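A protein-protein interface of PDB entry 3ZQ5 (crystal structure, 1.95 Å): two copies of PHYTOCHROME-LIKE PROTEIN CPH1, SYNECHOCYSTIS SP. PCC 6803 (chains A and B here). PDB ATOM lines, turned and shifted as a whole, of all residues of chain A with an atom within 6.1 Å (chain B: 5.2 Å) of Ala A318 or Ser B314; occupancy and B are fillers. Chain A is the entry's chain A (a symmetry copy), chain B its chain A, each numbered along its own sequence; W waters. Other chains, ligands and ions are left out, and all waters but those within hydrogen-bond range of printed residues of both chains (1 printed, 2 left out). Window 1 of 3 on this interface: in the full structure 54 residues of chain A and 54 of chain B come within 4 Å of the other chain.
Ser A314 touches Ser B317, and with the chains exchanged Ser A317 touches Ser B314.
Ser A314 touches Ala B318, and with the chains exchanged Ala A318 touches Ser B314.
Asn A315 touches Ala B318, and with the chains exchanged Ala A318 touches Asn B315.
Ala B318 touches its own counterpart, Ala A318.
6 positions are printed for both chains.
Water W1 lies within hydrogen-bond range of the backbone carbonyl oxygen (O) of Asn A315 (2.9 Å), the guanidinium group (NH1) of Arg B148 (3.1 Å) and the backbone NH (N) of Gln A319 (3.4 Å).
OE1 of Gln A319 sits close to NH2 of Arg B148 (2.3 Å).
OG1 of Thr A322 sits at hydrogen-bond distance from ND2 of Asn B315 (3.0 Å).
OG1 of Thr A322 is in hydrogen-bond range of NH1 of Arg B148, 3.4 Å away.
The side-chain hydroxyl (OG) of Ser B314 sits at hydrogen-bond distance from the side-chain carboxylate (OD2) of Asp A321 (2.6 Å).
The backbone carbonyl oxygen (O) of Ala A318 is in hydrogen-bond range of the side-chain hydroxyl (OG1) of Thr A322 (2.7 Å).
O of Phe B313 is in hydrogen-bond range of OG of Ser B317 (3.5 Å).
The backbone carbonyl oxygen (O) of Val B311 lies within hydrogen-bond range of the side-chain amide nitrogen (ND2) of Asn B315 (2.8 Å).
The side-chain carboxylate of Glu A323 is in hydrogen-bond range of the side-chain amide nitrogen of Gln A319 (2.7 Å).
The backbone carbonyl oxygen (O) of Phe A313 sits at hydrogen-bond distance from the side-chain hydroxyl (OG) of Ser A317, at 3.5 Å.
The guanidinium group of Arg B148 lies within hydrogen-bond range of the side-chain amide oxygen of Asn B315, 3.0 Å away.
Among the printed residues, merely in contact across the chains: Ser A314 with Ala B318 (3.4 Å), Ala A318 with Ser B314 (3.4 Å), Ser A314 with Ser B317 (3.8 Å), Ser A317 with Ser B314 (3.8 Å), Ala A318 with Ala B318 (3.8 Å), Ala A318 with Asn B315 (3.8 Å), Asn A315 with Ala B318 (3.8 Å) and Asp A321 with Val B311 (3.8 Å).
Printed residues of chain B within 4 Å of Ser A314: Ser B317 (3.8 Å) and Ala B318 (3.4 Å).
Printed residues of chain B within 4 Å of Ser A317: Ser B314 (3.8 Å).
Ala A318 touches just these residues of chain B: Ser B314, Asn B315 and Ala B318.
Of chain A, only Ser A317, Ala A318 and Asp A321 come within 4 Å of Ser B314.
Of the printed residues of chain A, Asn B315 touches Ala A318 (3.8 Å) and Thr A322 (3.0 Å).
Printed residues of chain A within 4 Å of Ser B317: Ser A314 (3.8 Å).
Printed residues of chain A within 4 Å of Ala B318: Ser A314 (3.4 Å), Asn A315 (3.8 Å) and Ala A318 (3.8 Å).
The nearest residue of chain A that does not touch Ser B314 is Ser A314 (5.0 Å).
The nearest printed residue of chain A that does not touch Arg B148 is Ala A318 (4.3 Å).
Of the 11 printed residues of chain B, 6 touch a printed residue of chain A.
Printed residues of chain B that touch a printed residue of chain A: Arg B148, Val B311, Ser B314, Asn B315, Ser B317 and Ala B318.
Hydrophobic or aromatic side chains of chain B within 4 Å of the printed part of chain A: Val B311 and Ala B318.
Of the 11 printed residues of chain A, 7 touch a printed residue of chain B.
Among the printed residues, no Asp or Glu carboxylate lies within 4 Å of a Lys or Arg side-chain nitrogen of the other chain.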
ATOM      1  N   PHE A 313      26.658  -0.040 -21.491  1.00  0.00           N
ATOM      2  CA  PHE A 313      27.627   0.745 -22.238  1.00  0.00           C
ATOM      3  C   PHE A 313      27.297   2.240 -22.259  1.00  0.00           C
ATOM      4  O   PHE A 313      28.191   3.074 -22.176  1.00  0.00           O
ATOM      5  CB  PHE A 313      27.767   0.228 -23.667  1.00  0.00           C
ATOM      6  CG  PHE A 313      28.762   0.981 -24.473  1.00  0.00           C
ATOM      7  CD1 PHE A 313      30.059   1.130 -24.022  1.00  0.00           C
ATOM      8  CD2 PHE A 313      28.417   1.526 -25.688  1.00  0.00           C
ATOM      9  CE1 PHE A 313      30.995   1.827 -24.765  1.00  0.00           C
ATOM     10  CE2 PHE A 313      29.356   2.229 -26.435  1.00  0.00           C
ATOM     11  CZ  PHE A 313      30.642   2.374 -25.962  1.00  0.00           C
ATOM     12  N   SER A 314      26.016   2.569 -22.364  1.00  0.00           N
ATOM     13  CA  SER A 314      25.561   3.936 -22.221  1.00  0.00           C
ATOM     14  C   SER A 314      25.977   4.511 -20.869  1.00  0.00           C
ATOM     15  O   SER A 314      26.435   5.652 -20.778  1.00  0.00           O
ATOM     16  CB  SER A 314      24.035   3.982 -22.393  1.00  0.00           C
ATOM     17  OG  SER A 314      23.559   5.302 -22.299  1.00  0.00           O
ATOM     18  N   ASN A 315      25.824   3.713 -19.810  1.00  0.00           N
ATOM     19  CA  ASN A 315      26.303   4.108 -18.490  1.00  0.00           C
ATOM     20  C   ASN A 315      27.842   4.222 -18.383  1.00  0.00           C
ATOM     21  O   ASN A 315      28.356   5.091 -17.678  1.00  0.00           O
ATOM     22  CB  ASN A 315      25.753   3.172 -17.424  1.00  0.00           C
ATOM     23  CG  ASN A 315      24.319   3.478 -17.086  1.00  0.00           C
ATOM     24  OD1 ASN A 315      24.059   4.297 -16.226  1.00  0.00           O
ATOM     25  ND2 ASN A 315      23.375   2.850 -17.798  1.00  0.00           N
ATOM     26  N   ILE A 316      28.564   3.378 -19.109  1.00  0.00           N
ATOM     27  CA  ILE A 316      30.023   3.481 -19.185  1.00  0.00           C
ATOM     28  C   ILE A 316      30.464   4.814 -19.835  1.00  0.00           C
ATOM     29  O   ILE A 316      31.365   5.459 -19.339  1.00  0.00           O
ATOM     30  CB  ILE A 316      30.651   2.277 -19.960  1.00  0.00           C
ATOM     31  CG1 ILE A 316      30.526   0.988 -19.146  1.00  0.00           C
ATOM     32  CG2 ILE A 316      32.120   2.566 -20.330  1.00  0.00           C
ATOM     33  CD1 ILE A 316      30.865  -0.330 -19.930  1.00  0.00           C
ATOM     34  N   SER A 317      29.827   5.241 -20.924  1.00  0.00           N
ATOM     35  CA  SER A 317      30.154   6.553 -21.511  1.00  0.00           C
ATOM     36  C   SER A 317      29.968   7.682 -20.524  1.00  0.00           C
ATOM     37  O   SER A 317      30.808   8.545 -20.427  1.00  0.00           O
ATOM     38  CB  SER A 317      29.330   6.851 -22.758  1.00  0.00           C
ATOM     39  OG  SER A 317      29.606   5.869 -23.722  1.00  0.00           O
ATOM     40  N   ALA A 318      28.864   7.652 -19.789  1.00  0.00           N
ATOM     41  CA  ALA A 318      28.562   8.665 -18.804  1.00  0.00           C
ATOM     42  C   ALA A 318      29.568   8.654 -17.660  1.00  0.00           C
ATOM     43  O   ALA A 318      29.953   9.711 -17.155  1.00  0.00           O
ATOM     44  CB  ALA A 318      27.175   8.465 -18.256  1.00  0.00           C
ATOM     45  N   GLN A 319      29.973   7.462 -17.246  1.00  0.00           N
ATOM     46  CA  GLN A 319      30.963   7.316 -16.180  1.00  0.00           C
ATOM     47  C   GLN A 319      32.320   7.890 -16.620  1.00  0.00           C
ATOM     48  O   GLN A 319      32.922   8.628 -15.876  1.00  0.00           O
ATOM     49  CB  GLN A 319      31.097   5.842 -15.783  1.00  0.00           C
ATOM     50  CG  GLN A 319      32.119   5.570 -14.696  1.00  0.00           C
ATOM     51  CD  GLN A 319      31.701   6.102 -13.375  1.00  0.00           C
ATOM     52  OE1 GLN A 319      30.519   6.267 -13.120  1.00  0.00           O
ATOM     53  NE2 GLN A 319      32.658   6.374 -12.520  1.00  0.00           N
ATOM     54  N   GLU A 320      32.766   7.561 -17.828  1.00  0.00           N
ATOM     55  CA  GLU A 320      34.005   8.096 -18.400  1.00  0.00           C
ATOM     56  C   GLU A 320      33.969   9.632 -18.461  1.00  0.00           C
ATOM     57  O   GLU A 320      34.907  10.310 -18.026  1.00  0.00           O
ATOM     58  CB  GLU A 320      34.236   7.549 -19.823  1.00  0.00           C
ATOM     59  CG  GLU A 320      34.804   6.126 -19.923  1.00  0.00           C
ATOM     60  CD  GLU A 320      34.817   5.560 -21.373  1.00  0.00           C
ATOM     61  OE1 GLU A 320      34.327   6.241 -22.307  1.00  0.00           O
ATOM     62  OE2 GLU A 320      35.328   4.432 -21.583  1.00  0.00           O
ATOM     63  N   ASP A 321      32.869  10.188 -18.977  1.00  0.00           N
ATOM     64  CA  ASP A 321      32.709  11.657 -19.004  1.00  0.00           C
ATOM     65  C   ASP A 321      32.700  12.300 -17.610  1.00  0.00           C
ATOM     66  O   ASP A 321      33.307  13.368 -17.401  1.00  0.00           O
ATOM     67  CB  ASP A 321      31.445  12.040 -19.812  1.00  0.00           C
ATOM     68  CG  ASP A 321      31.523  11.579 -21.270  1.00  0.00           C
ATOM     69  OD1 ASP A 321      32.646  11.355 -21.772  1.00  0.00           O
ATOM     70  OD2 ASP A 321      30.469  11.403 -21.912  1.00  0.00           O
ATOM     71  N   THR A 322      32.017  11.659 -16.664  1.00  0.00           N
ATOM     72  CA  THR A 322      31.966  12.121 -15.272  1.00  0.00           C
ATOM     73  C   THR A 322      33.327  12.107 -14.565  1.00  0.00           C
ATOM     74  O   THR A 322      33.670  13.054 -13.870  1.00  0.00           O
ATOM     75  CB  THR A 322      30.945  11.280 -14.451  1.00  0.00           C
ATOM     76  OG1 THR A 322      29.660  11.373 -15.055  1.00  0.00           O
ATOM     77  CG2 THR A 322      30.846  11.748 -12.994  1.00  0.00           C
ATOM     78  N   GLU A 323      34.109  11.041 -14.760  1.00  0.00           N
ATOM     79  CA  GLU A 323      35.432  10.946 -14.168  1.00  0.00           C
ATOM     80  C   GLU A 323      36.370  11.990 -14.751  1.00  0.00           C
ATOM     81  O   GLU A 323      37.166  12.567 -14.023  1.00  0.00           O
ATOM     82  CB  GLU A 323      36.037   9.539 -14.353  1.00  0.00           C
ATOM     83  CG  GLU A 323      35.258   8.477 -13.582  1.00  0.00           C
ATOM     84  CD  GLU A 323      35.920   7.111 -13.546  1.00  0.00           C
ATOM     85  OE1 GLU A 323      37.061   6.962 -14.027  1.00  0.00           O
ATOM     86  OE2 GLU A 323      35.274   6.177 -13.034  1.00  0.00           O
ATOM     87  N   ARG B 148      23.766  11.408  -9.613  1.00  0.00           N
ATOM     88  CA  ARG B 148      24.257  10.080  -9.886  1.00  0.00           C
ATOM     89  C   ARG B 148      23.965   9.129  -8.731  1.00  0.00           C
ATOM     90  O   ARG B 148      23.920   7.929  -8.929  1.00  0.00           O
ATOM     91  CB  ARG B 148      25.750  10.127 -10.220  1.00  0.00           C
ATOM     92  CG  ARG B 148      26.018  10.793 -11.569  1.00  0.00           C
ATOM     93  CD  ARG B 148      27.496  11.094 -11.767  1.00  0.00           C
ATOM     94  NE  ARG B 148      28.317   9.913 -11.513  1.00  0.00           N
ATOM     95  CZ  ARG B 148      28.471   8.887 -12.351  1.00  0.00           C
ATOM     96  NH1 ARG B 148      27.861   8.855 -13.539  1.00  0.00           N
ATOM     97  NH2 ARG B 148      29.247   7.874 -11.989  1.00  0.00           N
ATOM     98  N   GLY B 309      27.719  21.180 -19.276  1.00  0.00           N
ATOM     99  CA  GLY B 309      26.448  20.850 -19.906  1.00  0.00           C
ATOM    100  C   GLY B 309      26.522  19.547 -20.666  1.00  0.00           C
ATOM    101  O   GLY B 309      25.599  18.737 -20.617  1.00  0.00           O
ATOM    102  N   ARG B 310      27.631  19.326 -21.346  1.00  0.00           N
ATOM    103  CA  ARG B 310      27.828  18.086 -22.075  1.00  0.00           C
ATOM    104  C   ARG B 310      28.094  16.845 -21.226  1.00  0.00           C
ATOM    105  O   ARG B 310      27.679  15.754 -21.603  1.00  0.00           O
ATOM    106  CB  ARG B 310      28.886  18.285 -23.168  1.00  0.00           C
ATOM    107  CG  ARG B 310      28.297  19.211 -24.245  1.00  0.00           C
ATOM    108  CD  ARG B 310      29.164  19.460 -25.467  1.00  0.00           C
ATOM    109  NE  ARG B 310      28.393  20.202 -26.484  1.00  0.00           N
ATOM    110  CZ  ARG B 310      28.721  20.300 -27.773  1.00  0.00           C
ATOM    111  NH1 ARG B 310      29.821  19.714 -28.253  1.00  0.00           N
ATOM    112  NH2 ARG B 310      27.936  20.990 -28.597  1.00  0.00           N
ATOM    113  N   VAL B 311      28.751  17.008 -20.082  1.00  0.00           N
ATOM    114  CA  VAL B 311      28.877  15.924 -19.121  1.00  0.00           C
ATOM    115  C   VAL B 311      27.535  15.555 -18.467  1.00  0.00           C
ATOM    116  O   VAL B 311      27.219  14.381 -18.299  1.00  0.00           O
ATOM    117  CB  VAL B 311      29.897  16.255 -18.030  1.00  0.00           C
ATOM    118  CG1 VAL B 311      29.919  15.143 -16.984  1.00  0.00           C
ATOM    119  CG2 VAL B 311      31.270  16.421 -18.673  1.00  0.00           C
ATOM    120  N   VAL B 312      26.743  16.556 -18.110  1.00  0.00           N
ATOM    121  CA  VAL B 312      25.406  16.287 -17.627  1.00  0.00           C
ATOM    122  C   VAL B 312      24.575  15.609 -18.722  1.00  0.00           C
ATOM    123  O   VAL B 312      23.838  14.666 -18.452  1.00  0.00           O
ATOM    124  CB  VAL B 312      24.701  17.559 -17.095  1.00  0.00           C
ATOM    125  CG1 VAL B 312      23.291  17.223 -16.592  1.00  0.00           C
ATOM    126  CG2 VAL B 312      25.524  18.190 -15.939  1.00  0.00           C
ATOM    127  N   PHE B 313      24.691  16.082 -19.962  1.00  0.00           N
ATOM    128  CA  PHE B 313      23.929  15.496 -21.052  1.00  0.00           C
ATOM    129  C   PHE B 313      24.291  14.032 -21.317  1.00  0.00           C
ATOM    130  O   PHE B 313      23.421  13.221 -21.610  1.00  0.00           O
ATOM    131  CB  PHE B 313      24.094  16.308 -22.334  1.00  0.00           C
ATOM    132  CG  PHE B 313      23.318  15.766 -23.480  1.00  0.00           C
ATOM    133  CD1 PHE B 313      21.957  15.556 -23.366  1.00  0.00           C
ATOM    134  CD2 PHE B 313      23.933  15.484 -24.676  1.00  0.00           C
ATOM    135  CE1 PHE B 313      21.224  15.055 -24.427  1.00  0.00           C
ATOM    136  CE2 PHE B 313      23.199  14.978 -25.743  1.00  0.00           C
ATOM    137  CZ  PHE B 313      21.844  14.766 -25.606  1.00  0.00           C
ATOM    138  N   SER B 314      25.571  13.702 -21.205  1.00  0.00           N
ATOM    139  CA  SER B 314      26.016  12.326 -21.259  1.00  0.00           C
ATOM    140  C   SER B 314      25.328  11.488 -20.184  1.00  0.00           C
ATOM    141  O   SER B 314      24.887  10.364 -20.441  1.00  0.00           O
ATOM    142  CB  SER B 314      27.544  12.281 -21.098  1.00  0.00           C
ATOM    143  OG  SER B 314      28.018  10.960 -21.184  1.00  0.00           O
ATOM    144  N   ASN B 315      25.225  12.039 -18.973  1.00  0.00           N
ATOM    145  CA  ASN B 315      24.478  11.385 -17.905  1.00  0.00           C
ATOM    146  C   ASN B 315      22.956  11.287 -18.165  1.00  0.00           C
ATOM    147  O   ASN B 315      22.321  10.301 -17.791  1.00  0.00           O
ATOM    148  CB  ASN B 315      24.758  12.060 -16.571  1.00  0.00           C
ATOM    149  CG  ASN B 315      26.089  11.656 -16.000  1.00  0.00           C
ATOM    150  OD1 ASN B 315      26.174  10.667 -15.297  1.00  0.00           O
ATOM    151  ND2 ASN B 315      27.152  12.398 -16.337  1.00  0.00           N
ATOM    152  N   ILE B 316      22.390  12.283 -18.836  1.00  0.00           N
ATOM    153  CA  ILE B 316      20.987  12.233 -19.250  1.00  0.00           C
ATOM    154  C   ILE B 316      20.732  11.079 -20.248  1.00  0.00           C
ATOM    155  O   ILE B 316      19.759  10.365 -20.110  1.00  0.00           O
ATOM    156  CB  ILE B 316      20.516  13.588 -19.872  1.00  0.00           C
ATOM    157  CG1 ILE B 316      20.428  14.673 -18.795  1.00  0.00           C
ATOM    158  CG2 ILE B 316      19.171  13.419 -20.607  1.00  0.00           C
ATOM    159  CD1 ILE B 316      20.239  16.134 -19.337  1.00  0.00           C
ATOM    160  N   SER B 317      21.602  10.878 -21.236  1.00  0.00           N
ATOM    161  CA  SER B 317      21.442   9.728 -22.145  1.00  0.00           C
ATOM    162  C   SER B 317      21.435   8.412 -21.404  1.00  0.00           C
ATOM    163  O   SER B 317      20.615   7.567 -21.679  1.00  0.00           O
ATOM    164  CB  SER B 317      22.527   9.682 -23.215  1.00  0.00           C
ATOM    165  OG  SER B 317      22.446  10.852 -23.986  1.00  0.00           O
ATOM    166  N   ALA B 318      22.349   8.258 -20.456  1.00  0.00           N
ATOM    167  CA  ALA B 318      22.452   7.053 -19.666  1.00  0.00           C
ATOM    168  C   ALA B 318      21.220   6.846 -18.795  1.00  0.00           C
ATOM    169  O   ALA B 318      20.759   5.714 -18.622  1.00  0.00           O
ATOM    170  CB  ALA B 318      23.680   7.100 -18.797  1.00  0.00           C
HETATM  171  O   HOH W   1      27.706   6.147 -15.086  1.00  0.00           O
